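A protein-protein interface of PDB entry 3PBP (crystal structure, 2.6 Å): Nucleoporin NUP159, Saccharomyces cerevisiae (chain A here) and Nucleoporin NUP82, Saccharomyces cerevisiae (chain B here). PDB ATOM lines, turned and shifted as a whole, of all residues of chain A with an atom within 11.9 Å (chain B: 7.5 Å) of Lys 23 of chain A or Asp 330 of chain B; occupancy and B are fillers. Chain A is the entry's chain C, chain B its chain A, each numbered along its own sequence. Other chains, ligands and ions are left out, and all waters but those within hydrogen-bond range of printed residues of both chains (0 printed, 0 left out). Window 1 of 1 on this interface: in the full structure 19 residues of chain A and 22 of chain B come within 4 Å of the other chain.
ND2 of Asn 288 of chain B sits close to NZ of Lys 30 of chain A, at 3.3 Å.
Of the printed residues of chain B, Lys 23 of chain A touches Asp 330 and Leu 331. Of the printed residues of chain A, Asp 330 of chain B touches Lys 22 (3.4 Å), Lys 23 (3.9 Å) and Gly 26 (3.7 Å). No residue of chain A comes within 4 Å of Lys 329 of chain B. Val 349 of chain B touches just these residues of chain A: Gly 26 and Phe 29. Of the printed residues of chain B, Lys 22 of chain A touches Asp 330. Of the printed residues of chain A, Leu 402 of chain B touches Thr 21 (3.5 Å), Gln 24 (3.3 Å) and Ile 25 (3.5 Å). The nearest residue of chain B that does not touch Lys 23 of chain A is Asn 345 of chain B (5.6 Å). The nearest residue of chain A that does not touch Asp 330 of chain B is Lys 30 of chain A (4.1 Å).
Hydrophobic or aromatic side chains of chain A that line the printed part of chain B: Met 19, Ile 25 and Phe 29. Of the 17 printed residues of chain B, 7 touch a printed residue of chain A. Hydrophobic or aromatic side chains of chain B that line the printed part of chain A: Phe 328, Leu 331, Val 349 and Leu 402. Among the printed residues, 12 pairs touch across the chains. Among the printed residues, no Asp or Glu carboxylate lies within 4 Å of a Lys or Arg side-chain nitrogen of the other chain.
Among the printed residues, merely in contact across the chains: Met 19 of chain A with Glu 332 of chain B (3.4 Å), Thr 21 of chain A with Leu 402 of chain B (3.5 Å), Lys 22 of chain A with Asp 330 of chain B (3.4 Å), Lys 23 of chain A with Asp 330 of chain B (3.9 Å), Lys 23 of chain A with Leu 331 of chain B (3.6 Å), Gln 24 of chain A with Leu 402 of chain B (3.3 Å), Ile 25 of chain A with Phe 328 of chain B (3.8 Å), Ile 25 of chain A with Leu 402 of chain B (3.5 Å), Gly 26 of chain A with Asp 330 of chain B (3.7 Å), Gly 26 of chain A with Val 349 of chain B (3.9 Å) and Phe 29 of chain A with Val 349 of chain B (3.2 Å).
The backbone NH of Asn 288 of chain B sits at hydrogen-bond distance from the backbone carbonyl oxygen of Leu 348 of chain B, 2.9 Å away. O of Phe 328 of chain B sits at hydrogen-bond distance from N of Val 349 of chain B. The backbone carbonyl oxygen (O) of Leu 331 of chain B sits close to the side-chain amino group (NZ) of Lys 329 of chain B, 3.4 Å away. OD2 of Asp 330 of chain B lies within hydrogen-bond range of OG of Ser 347 of chain B, 2.6 Å away. The side-chain amide nitrogen of Asn 345 of chain B sits at hydrogen-bond distance from the backbone carbonyl oxygen of Glu 332 of chain B, at 2.9 Å. The backbone carbonyl oxygen (O) of Leu 17 of chain A lies within hydrogen-bond range of the side-chain hydroxyl (OG1) of Thr 21 of chain A (2.8 Å).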
ATOM      1  N   GLU A  14      12.027   3.129  12.853  1.00  0.00           N
ATOM      2  CA  GLU A  14      13.404   2.958  13.283  1.00  0.00           C
ATOM      3  C   GLU A  14      13.646   1.522  13.788  1.00  0.00           C
ATOM      4  O   GLU A  14      14.626   0.875  13.403  1.00  0.00           O
ATOM      5  CB  GLU A  14      13.704   3.988  14.378  1.00  0.00           C
ATOM      6  CG  GLU A  14      15.049   3.839  15.089  1.00  0.00           C
ATOM      7  CD  GLU A  14      15.287   4.936  16.138  1.00  0.00           C
ATOM      8  OE1 GLU A  14      15.376   6.120  15.742  1.00  0.00           O
ATOM      9  OE2 GLU A  14      15.379   4.616  17.349  1.00  0.00           O
ATOM     10  N   VAL A  15      12.749   1.020  14.633  1.00  0.00           N
ATOM     11  CA  VAL A  15      12.884  -0.331  15.172  1.00  0.00           C
ATOM     12  C   VAL A  15      12.730  -1.398  14.083  1.00  0.00           C
ATOM     13  O   VAL A  15      13.507  -2.365  14.028  1.00  0.00           O
ATOM     14  CB  VAL A  15      11.843  -0.588  16.286  1.00  0.00           C
ATOM     15  CG1 VAL A  15      11.894  -2.042  16.724  1.00  0.00           C
ATOM     16  CG2 VAL A  15      12.109   0.319  17.472  1.00  0.00           C
ATOM     17  N   GLY A  16      11.721  -1.224  13.227  1.00  0.00           N
ATOM     18  CA  GLY A  16      11.488  -2.163  12.143  1.00  0.00           C
ATOM     19  C   GLY A  16      12.691  -2.243  11.209  1.00  0.00           C
ATOM     20  O   GLY A  16      13.034  -3.315  10.686  1.00  0.00           O
ATOM     21  N   LEU A  17      13.337  -1.104  10.987  1.00  0.00           N
ATOM     22  CA  LEU A  17      14.503  -1.061  10.123  1.00  0.00           C
ATOM     23  C   LEU A  17      15.635  -1.887  10.730  1.00  0.00           C
ATOM     24  O   LEU A  17      16.303  -2.656  10.026  1.00  0.00           O
ATOM     25  CB  LEU A  17      14.955   0.386   9.923  1.00  0.00           C
ATOM     26  CG  LEU A  17      14.032   1.263   9.082  1.00  0.00           C
ATOM     27  CD1 LEU A  17      14.465   2.721   9.180  1.00  0.00           C
ATOM     28  CD2 LEU A  17      14.070   0.787   7.644  1.00  0.00           C
ATOM     29  N   ALA A  18      15.845  -1.718  12.035  1.00  0.00           N
ATOM     30  CA  ALA A  18      16.883  -2.460  12.752  1.00  0.00           C
ATOM     31  C   ALA A  18      16.605  -3.960  12.683  1.00  0.00           C
ATOM     32  O   ALA A  18      17.510  -4.751  12.423  1.00  0.00           O
ATOM     33  CB  ALA A  18      16.938  -2.018  14.192  1.00  0.00           C
ATOM     34  N   MET A  19      15.354  -4.350  12.916  1.00  0.00           N
ATOM     35  CA  MET A  19      14.989  -5.758  12.854  1.00  0.00           C
ATOM     36  C   MET A  19      15.264  -6.323  11.474  1.00  0.00           C
ATOM     37  O   MET A  19      15.761  -7.439  11.339  1.00  0.00           O
ATOM     38  CB  MET A  19      13.517  -5.934  13.195  1.00  0.00           C
ATOM     39  CG  MET A  19      13.231  -5.787  14.659  1.00  0.00           C
ATOM     40  SD  MET A  19      11.379  -5.772  15.020  1.00  0.00           S
ATOM     41  CE  MET A  19      10.869  -7.551  14.322  1.00  0.00           C
ATOM     42  N   ASN A  20      14.935  -5.544  10.450  1.00  0.00           N
ATOM     43  CA  ASN A  20      15.153  -5.963   9.077  1.00  0.00           C
ATOM     44  C   ASN A  20      16.645  -6.047   8.749  1.00  0.00           C
ATOM     45  O   ASN A  20      17.082  -6.942   8.020  1.00  0.00           O
ATOM     46  CB  ASN A  20      14.454  -5.002   8.122  1.00  0.00           C
ATOM     47  CG  ASN A  20      14.541  -5.458   6.671  1.00  0.00           C
ATOM     48  OD1 ASN A  20      15.521  -5.175   5.972  1.00  0.00           O
ATOM     49  ND2 ASN A  20      13.519  -6.182   6.215  1.00  0.00           N
ATOM     50  N   THR A  21      17.429  -5.116   9.283  1.00  0.00           N
ATOM     51  CA  THR A  21      18.865  -5.127   9.047  1.00  0.00           C
ATOM     52  C   THR A  21      19.455  -6.425   9.606  1.00  0.00           C
ATOM     53  O   THR A  21      20.290  -7.069   8.972  1.00  0.00           O
ATOM     54  CB  THR A  21      19.546  -3.923   9.726  1.00  0.00           C
ATOM     55  OG1 THR A  21      18.946  -2.715   9.255  1.00  0.00           O
ATOM     56  CG2 THR A  21      21.008  -3.889   9.400  1.00  0.00           C
ATOM     57  N   LYS A  22      19.002  -6.811  10.794  1.00  0.00           N
ATOM     58  CA  LYS A  22      19.478  -8.030  11.437  1.00  0.00           C
ATOM     59  C   LYS A  22      19.215  -9.274  10.594  1.00  0.00           C
ATOM     60  O   LYS A  22      20.005 -10.216  10.620  1.00  0.00           O
ATOM     61  CB  LYS A  22      18.829  -8.205  12.813  1.00  0.00           C
ATOM     62  CG  LYS A  22      19.318  -7.233  13.866  1.00  0.00           C
ATOM     63  CD  LYS A  22      18.690  -7.556  15.182  1.00  0.00           C
ATOM     64  CE  LYS A  22      19.236  -6.674  16.264  1.00  0.00           C
ATOM     65  NZ  LYS A  22      18.740  -7.077  17.616  1.00  0.00           N
ATOM     66  N   LYS A  23      18.104  -9.292   9.863  1.00  0.00           N
ATOM     67  CA  LYS A  23      17.804 -10.442   9.028  1.00  0.00           C
ATOM     68  C   LYS A  23      18.847 -10.518   7.942  1.00  0.00           C
ATOM     69  O   LYS A  23      19.396 -11.591   7.654  1.00  0.00           O
ATOM     70  CB  LYS A  23      16.429 -10.322   8.375  1.00  0.00           C
ATOM     71  CG  LYS A  23      15.279 -10.743   9.250  1.00  0.00           C
ATOM     72  CD  LYS A  23      13.968 -10.705   8.471  1.00  0.00           C
ATOM     73  CE  LYS A  23      12.790 -11.197   9.330  1.00  0.00           C
ATOM     74  NZ  LYS A  23      11.473 -11.129   8.611  1.00  0.00           N
ATOM     75  N   GLN A  24      19.112  -9.363   7.341  1.00  0.00           N
ATOM     76  CA  GLN A  24      20.078  -9.262   6.266  1.00  0.00           C
ATOM     77  C   GLN A  24      21.438  -9.700   6.757  1.00  0.00           C
ATOM     78  O   GLN A  24      22.187 -10.337   6.026  1.00  0.00           O
ATOM     79  CB  GLN A  24      20.118  -7.833   5.750  1.00  0.00           C
ATOM     80  CG  GLN A  24      18.775  -7.360   5.254  1.00  0.00           C
ATOM     81  CD  GLN A  24      18.830  -5.988   4.636  1.00  0.00           C
ATOM     82  OE1 GLN A  24      19.242  -5.009   5.284  1.00  0.00           O
ATOM     83  NE2 GLN A  24      18.412  -5.895   3.375  1.00  0.00           N
ATOM     84  N   ILE A  25      21.746  -9.361   8.003  1.00  0.00           N
ATOM     85  CA  ILE A  25      23.010  -9.736   8.619  1.00  0.00           C
ATOM     86  C   ILE A  25      22.992 -11.232   8.900  1.00  0.00           C
ATOM     87  O   ILE A  25      24.032 -11.864   9.004  1.00  0.00           O
ATOM     88  CB  ILE A  25      23.230  -8.966   9.943  1.00  0.00           C
ATOM     89  CG1 ILE A  25      23.555  -7.508   9.626  1.00  0.00           C
ATOM     90  CG2 ILE A  25      24.315  -9.633  10.779  1.00  0.00           C
ATOM     91  CD1 ILE A  25      23.966  -6.712  10.818  1.00  0.00           C
ATOM     92  N   GLY A  26      21.795 -11.790   9.020  1.00  0.00           N
ATOM     93  CA  GLY A  26      21.669 -13.211   9.267  1.00  0.00           C
ATOM     94  C   GLY A  26      22.142 -13.979   8.053  1.00  0.00           C
ATOM     95  O   GLY A  26      22.867 -14.971   8.176  1.00  0.00           O
ATOM     96  N   ASP A  27      21.734 -13.514   6.871  1.00  0.00           N
ATOM     97  CA  ASP A  27      22.118 -14.153   5.612  1.00  0.00           C
ATOM     98  C   ASP A  27      23.610 -13.996   5.372  1.00  0.00           C
ATOM     99  O   ASP A  27      24.275 -14.917   4.902  1.00  0.00           O
ATOM    100  CB  ASP A  27      21.355 -13.542   4.442  1.00  0.00           C
ATOM    101  CG  ASP A  27      19.849 -13.675   4.594  1.00  0.00           C
ATOM    102  OD1 ASP A  27      19.393 -14.783   4.967  1.00  0.00           O
ATOM    103  OD2 ASP A  27      19.126 -12.679   4.331  1.00  0.00           O
ATOM    104  N   PHE A  28      24.130 -12.821   5.700  1.00  0.00           N
ATOM    105  CA  PHE A  28      25.538 -12.550   5.530  1.00  0.00           C
ATOM    106  C   PHE A  28      26.358 -13.642   6.197  1.00  0.00           C
ATOM    107  O   PHE A  28      27.214 -14.244   5.568  1.00  0.00           O
ATOM    108  CB  PHE A  28      25.867 -11.183   6.127  1.00  0.00           C
ATOM    109  CG  PHE A  28      27.333 -10.849   6.130  1.00  0.00           C
ATOM    110  CD1 PHE A  28      28.217 -11.526   6.964  1.00  0.00           C
ATOM    111  CD2 PHE A  28      27.819  -9.821   5.334  1.00  0.00           C
ATOM    112  CE1 PHE A  28      29.560 -11.181   7.008  1.00  0.00           C
ATOM    113  CE2 PHE A  28      29.160  -9.468   5.368  1.00  0.00           C
ATOM    114  CZ  PHE A  28      30.034 -10.150   6.209  1.00  0.00           C
ATOM    115  N   PHE A  29      26.092 -13.911   7.468  1.00  0.00           N
ATOM    116  CA  PHE A  29      26.844 -14.934   8.183  1.00  0.00           C
ATOM    117  C   PHE A  29      26.499 -16.360   7.772  1.00  0.00           C
ATOM    118  O   PHE A  29      27.295 -17.275   7.982  1.00  0.00           O
ATOM    119  CB  PHE A  29      26.665 -14.769   9.688  1.00  0.00           C
ATOM    120  CG  PHE A  29      27.458 -13.642  10.269  1.00  0.00           C
ATOM    121  CD1 PHE A  29      28.842 -13.715  10.335  1.00  0.00           C
ATOM    122  CD2 PHE A  29      26.824 -12.498  10.749  1.00  0.00           C
ATOM    123  CE1 PHE A  29      29.585 -12.669  10.870  1.00  0.00           C
ATOM    124  CE2 PHE A  29      27.561 -11.444  11.286  1.00  0.00           C
ATOM    125  CZ  PHE A  29      28.940 -11.530  11.346  1.00  0.00           C
ATOM    126  N   LYS A  30      25.311 -16.555   7.204  1.00  0.00           N
ATOM    127  CA  LYS A  30      24.916 -17.880   6.739  1.00  0.00           C
ATOM    128  C   LYS A  30      25.757 -18.176   5.492  1.00  0.00           C
ATOM    129  O   LYS A  30      26.397 -19.228   5.381  1.00  0.00           O
ATOM    130  CB  LYS A  30      23.435 -17.903   6.367  1.00  0.00           C
ATOM    131  CG  LYS A  30      22.463 -17.857   7.525  1.00  0.00           C
ATOM    132  CD  LYS A  30      21.049 -17.630   6.994  1.00  0.00           C
ATOM    133  CE  LYS A  30      19.991 -17.725   8.072  1.00  0.00           C
ATOM    134  NZ  LYS A  30      19.977 -19.078   8.655  1.00  0.00           N
ATOM    135  N   ASN A  31      25.764 -17.221   4.567  1.00  0.00           N
ATOM    136  CA  ASN A  31      26.505 -17.348   3.319  1.00  0.00           C
ATOM    137  C   ASN A  31      27.951 -16.896   3.447  1.00  0.00           C
ATOM    138  O   ASN A  31      28.531 -16.395   2.488  1.00  0.00           O
ATOM    139  CB  ASN A  31      25.812 -16.540   2.220  1.00  0.00           C
ATOM    140  CG  ASN A  31      24.319 -16.817   2.157  1.00  0.00           C
ATOM    141  OD1 ASN A  31      23.898 -17.968   1.998  1.00  0.00           O
ATOM    142  ND2 ASN A  31      23.508 -15.763   2.290  1.00  0.00           N
ATOM    143  N   LEU A  32      28.519 -17.053   4.638  1.00  0.00           N
ATOM    144  CA  LEU A  32      29.910 -16.690   4.878  1.00  0.00           C
ATOM    145  C   LEU A  32      30.690 -17.943   5.265  1.00  0.00           C
ATOM    146  O   LEU A  32      31.872 -18.089   4.937  1.00  0.00           O
ATOM    147  CB  LEU A  32      30.029 -15.654   5.996  1.00  0.00           C
ATOM    148  CG  LEU A  32      31.477 -15.361   6.415  1.00  0.00           C
ATOM    149  CD1 LEU A  32      32.256 -14.827   5.233  1.00  0.00           C
ATOM    150  CD2 LEU A  32      31.504 -14.360   7.544  1.00  0.00           C
ATOM    151  N   SER B 236       3.673  -6.623  10.638  1.00  0.00           N
ATOM    152  CA  SER B 236       4.295  -7.659   9.822  1.00  0.00           C
ATOM    153  C   SER B 236       3.357  -8.840   9.556  1.00  0.00           C
ATOM    154  O   SER B 236       3.715  -9.776   8.840  1.00  0.00           O
ATOM    155  CB  SER B 236       5.573  -8.142  10.526  1.00  0.00           C
ATOM    156  OG  SER B 236       5.962  -9.436  10.109  1.00  0.00           O
ATOM    157  N   THR B 286      17.657 -22.988  15.939  1.00  0.00           N
ATOM    158  CA  THR B 286      18.425 -23.435  14.806  1.00  0.00           C
ATOM    159  C   THR B 286      19.793 -22.761  14.953  1.00  0.00           C
ATOM    160  O   THR B 286      19.863 -21.568  15.229  1.00  0.00           O
ATOM    161  CB  THR B 286      17.720 -22.979  13.540  1.00  0.00           C
ATOM    162  OG1 THR B 286      17.020 -24.086  12.983  1.00  0.00           O
ATOM    163  CG2 THR B 286      18.675 -22.437  12.547  1.00  0.00           C
ATOM    164  N   ASN B 288      22.745 -22.016  12.736  1.00  0.00           N
ATOM    165  CA  ASN B 288      23.237 -22.057  11.370  1.00  0.00           C
ATOM    166  C   ASN B 288      24.427 -21.141  11.091  1.00  0.00           C
ATOM    167  O   ASN B 288      24.374 -19.941  11.354  1.00  0.00           O
ATOM    168  CB  ASN B 288      22.089 -21.674  10.446  1.00  0.00           C
ATOM    169  CG  ASN B 288      22.337 -22.061   9.012  1.00  0.00           C
ATOM    170  OD1 ASN B 288      23.461 -22.346   8.615  1.00  0.00           O
ATOM    171  ND2 ASN B 288      21.282 -22.061   8.220  1.00  0.00           N
ATOM    172  N   LEU B 327      27.497 -17.002  18.725  1.00  0.00           N
ATOM    173  CA  LEU B 327      26.282 -16.943  17.926  1.00  0.00           C
ATOM    174  C   LEU B 327      25.593 -15.587  17.971  1.00  0.00           C
ATOM    175  O   LEU B 327      25.800 -14.810  18.893  1.00  0.00           O
ATOM    176  CB  LEU B 327      25.315 -18.015  18.417  1.00  0.00           C
ATOM    177  CG  LEU B 327      25.916 -19.395  18.677  1.00  0.00           C
ATOM    178  CD1 LEU B 327      24.862 -20.315  19.318  1.00  0.00           C
ATOM    179  CD2 LEU B 327      26.433 -19.960  17.379  1.00  0.00           C
ATOM    180  N   PHE B 328      24.758 -15.334  16.965  1.00  0.00           N
ATOM    181  CA  PHE B 328      23.999 -14.096  16.829  1.00  0.00           C
ATOM    182  C   PHE B 328      22.543 -14.397  16.430  1.00  0.00           C
ATOM    183  O   PHE B 328      22.295 -15.115  15.461  1.00  0.00           O
ATOM    184  CB  PHE B 328      24.658 -13.219  15.766  1.00  0.00           C
ATOM    185  CG  PHE B 328      23.881 -11.982  15.436  1.00  0.00           C
ATOM    186  CD1 PHE B 328      23.838 -10.903  16.330  1.00  0.00           C
ATOM    187  CD2 PHE B 328      23.181 -11.894  14.237  1.00  0.00           C
ATOM    188  CE1 PHE B 328      23.100  -9.749  16.024  1.00  0.00           C
ATOM    189  CE2 PHE B 328      22.450 -10.757  13.923  1.00  0.00           C
ATOM    190  CZ  PHE B 328      22.407  -9.679  14.817  1.00  0.00           C
ATOM    191  N   LYS B 329      21.586 -13.849  17.178  1.00  0.00           N
ATOM    192  CA  LYS B 329      20.157 -14.054  16.907  1.00  0.00           C
ATOM    193  C   LYS B 329      19.637 -13.032  15.890  1.00  0.00           C
ATOM    194  O   LYS B 329      19.454 -11.860  16.221  1.00  0.00           O
ATOM    195  CB  LYS B 329      19.377 -13.947  18.215  1.00  0.00           C
ATOM    196  CG  LYS B 329      17.885 -13.952  18.091  1.00  0.00           C
ATOM    197  CD  LYS B 329      17.295 -14.015  19.482  1.00  0.00           C
ATOM    198  CE  LYS B 329      15.913 -13.383  19.556  1.00  0.00           C
ATOM    199  NZ  LYS B 329      15.906 -11.892  19.406  1.00  0.00           N
ATOM    200  N   ASP B 330      19.405 -13.492  14.656  1.00  0.00           N
ATOM    201  CA  ASP B 330      18.943 -12.644  13.566  1.00  0.00           C
ATOM    202  C   ASP B 330      17.446 -12.416  13.463  1.00  0.00           C
ATOM    203  O   ASP B 330      17.016 -11.391  12.928  1.00  0.00           O
ATOM    204  CB  ASP B 330      19.430 -13.180  12.216  1.00  0.00           C
ATOM    205  CG  ASP B 330      18.931 -14.594  11.917  1.00  0.00           C
ATOM    206  OD1 ASP B 330      18.591 -14.886  10.739  1.00  0.00           O
ATOM    207  OD2 ASP B 330      18.896 -15.426  12.851  1.00  0.00           O
ATOM    208  N   LEU B 331      16.641 -13.359  13.943  1.00  0.00           N
ATOM    209  CA  LEU B 331      15.198 -13.187  13.860  1.00  0.00           C
ATOM    210  C   LEU B 331      14.600 -12.725  15.172  1.00  0.00           C
ATOM    211  O   LEU B 331      15.144 -12.993  16.242  1.00  0.00           O
ATOM    212  CB  LEU B 331      14.544 -14.480  13.409  1.00  0.00           C
ATOM    213  CG  LEU B 331      15.099 -14.961  12.071  1.00  0.00           C
ATOM    214  CD1 LEU B 331      14.249 -16.108  11.556  1.00  0.00           C
ATOM    215  CD2 LEU B 331      15.104 -13.819  11.082  1.00  0.00           C
ATOM    216  N   GLU B 332      13.494 -12.002  15.093  1.00  0.00           N
ATOM    217  CA  GLU B 332      12.838 -11.520  16.299  1.00  0.00           C
ATOM    218  C   GLU B 332      11.831 -12.570  16.790  1.00  0.00           C
ATOM    219  O   GLU B 332      10.928 -12.990  16.045  1.00  0.00           O
ATOM    220  CB  GLU B 332      12.125 -10.201  16.005  1.00  0.00           C
ATOM    221  CG  GLU B 332      11.582  -9.492  17.228  1.00  0.00           C
ATOM    222  CD  GLU B 332      12.659  -9.137  18.227  1.00  0.00           C
ATOM    223  OE1 GLU B 332      13.656  -8.498  17.825  1.00  0.00           O
ATOM    224  OE2 GLU B 332      12.504  -9.497  19.416  1.00  0.00           O
ATOM    225  N   MET B 333      11.992 -13.014  18.032  1.00  0.00           N
ATOM    226  CA  MET B 333      11.078 -14.000  18.576  1.00  0.00           C
ATOM    227  C   MET B 333       9.777 -13.331  18.968  1.00  0.00           C
ATOM    228  O   MET B 333       9.706 -12.112  19.144  1.00  0.00           O
ATOM    229  CB  MET B 333      11.637 -14.639  19.842  1.00  0.00           C
ATOM    230  CG  MET B 333      12.931 -15.412  19.712  1.00  0.00           C
ATOM    231  SD  MET B 333      13.602 -15.849  21.528  1.00  0.00           S
ATOM    232  CE  MET B 333      12.289 -17.214  21.998  1.00  0.00           C
ATOM    233  N   TYR B 344       9.843 -20.663  16.025  1.00  0.00           N
ATOM    234  CA  TYR B 344       9.405 -19.555  15.192  1.00  0.00           C
ATOM    235  C   TYR B 344      10.388 -18.454  15.428  1.00  0.00           C
ATOM    236  O   TYR B 344      10.446 -17.856  16.492  1.00  0.00           O
ATOM    237  CB  TYR B 344       7.992 -19.056  15.526  1.00  0.00           C
ATOM    238  CG  TYR B 344       7.630 -17.855  14.680  1.00  0.00           C
ATOM    239  CD1 TYR B 344       7.498 -17.965  13.288  1.00  0.00           C
ATOM    240  CD2 TYR B 344       7.559 -16.580  15.244  1.00  0.00           C
ATOM    241  CE1 TYR B 344       7.323 -16.830  12.475  1.00  0.00           C
ATOM    242  CE2 TYR B 344       7.385 -15.439  14.444  1.00  0.00           C
ATOM    243  CZ  TYR B 344       7.274 -15.572  13.059  1.00  0.00           C
ATOM    244  OH  TYR B 344       7.162 -14.439  12.276  1.00  0.00           O
ATOM    245  N   ASN B 345      11.179 -18.201  14.414  1.00  0.00           N
ATOM    246  CA  ASN B 345      12.202 -17.205  14.519  1.00  0.00           C
ATOM    247  C   ASN B 345      13.156 -17.560  15.648  1.00  0.00           C
ATOM    248  O   ASN B 345      13.879 -16.699  16.163  1.00  0.00           O
ATOM    249  CB  ASN B 345      11.562 -15.831  14.687  1.00  0.00           C
ATOM    250  CG  ASN B 345      10.882 -15.368  13.414  1.00  0.00           C
ATOM    251  OD1 ASN B 345      10.822 -16.109  12.430  1.00  0.00           O
ATOM    252  ND2 ASN B 345      10.366 -14.146  13.426  1.00  0.00           N
ATOM    253  N   ASN B 346      13.150 -18.836  16.032  1.00  0.00           N
ATOM    254  CA  ASN B 346      14.076 -19.333  17.048  1.00  0.00           C
ATOM    255  C   ASN B 346      15.317 -19.639  16.221  1.00  0.00           C
ATOM    256  O   ASN B 346      15.663 -20.797  15.990  1.00  0.00           O
ATOM    257  CB  ASN B 346      13.550 -20.618  17.713  1.00  0.00           C
ATOM    258  CG  ASN B 346      12.431 -20.352  18.728  1.00  0.00           C
ATOM    259  OD1 ASN B 346      12.188 -21.159  19.596  1.00  0.00           O
ATOM    260  ND2 ASN B 346      11.754 -19.223  18.606  1.00  0.00           N
ATOM    261  N   SER B 347      15.974 -18.574  15.774  1.00  0.00           N
ATOM    262  CA  SER B 347      17.128 -18.691  14.904  1.00  0.00           C
ATOM    263  C   SER B 347      18.405 -18.022  15.369  1.00  0.00           C
ATOM    264  O   SER B 347      18.413 -16.850  15.695  1.00  0.00           O
ATOM    265  CB  SER B 347      16.766 -18.142  13.518  1.00  0.00           C
ATOM    266  OG  SER B 347      17.933 -17.882  12.754  1.00  0.00           O
ATOM    267  N   LEU B 348      19.486 -18.789  15.375  1.00  0.00           N
ATOM    268  CA  LEU B 348      20.799 -18.296  15.745  1.00  0.00           C
ATOM    269  C   LEU B 348      21.751 -18.549  14.576  1.00  0.00           C
ATOM    270  O   LEU B 348      21.663 -19.564  13.877  1.00  0.00           O
ATOM    271  CB  LEU B 348      21.322 -19.016  16.979  1.00  0.00           C
ATOM    272  CG  LEU B 348      20.691 -18.645  18.307  1.00  0.00           C
ATOM    273  CD1 LEU B 348      21.281 -19.527  19.381  1.00  0.00           C
ATOM    274  CD2 LEU B 348      20.946 -17.177  18.601  1.00  0.00           C
ATOM    275  N   VAL B 349      22.671 -17.625  14.379  1.00  0.00           N
ATOM    276  CA  VAL B 349      23.630 -17.727  13.304  1.00  0.00           C
ATOM    277  C   VAL B 349      25.041 -17.754  13.873  1.00  0.00           C
ATOM    278  O   VAL B 349      25.340 -17.015  14.800  1.00  0.00           O
ATOM    279  CB  VAL B 349      23.459 -16.520  12.356  1.00  0.00           C
ATOM    280  CG1 VAL B 349      24.560 -16.488  11.336  1.00  0.00           C
ATOM    281  CG2 VAL B 349      22.115 -16.612  11.661  1.00  0.00           C
ATOM    282  N   LEU B 402      24.840  -2.540   5.894  1.00  0.00           N
ATOM    283  CA  LEU B 402      25.609  -3.778   5.896  1.00  0.00           C
ATOM    284  C   LEU B 402      27.041  -3.685   5.370  1.00  0.00           C
ATOM    285  O   LEU B 402      27.887  -4.494   5.739  1.00  0.00           O
ATOM    286  CB  LEU B 402      24.847  -4.846   5.113  1.00  0.00           C
ATOM    287  CG  LEU B 402      23.992  -5.830   5.916  1.00  0.00           C
ATOM    288  CD1 LEU B 402      23.269  -5.117   7.031  1.00  0.00           C
ATOM    289  CD2 LEU B 402      23.010  -6.503   4.993  1.00  0.00           C
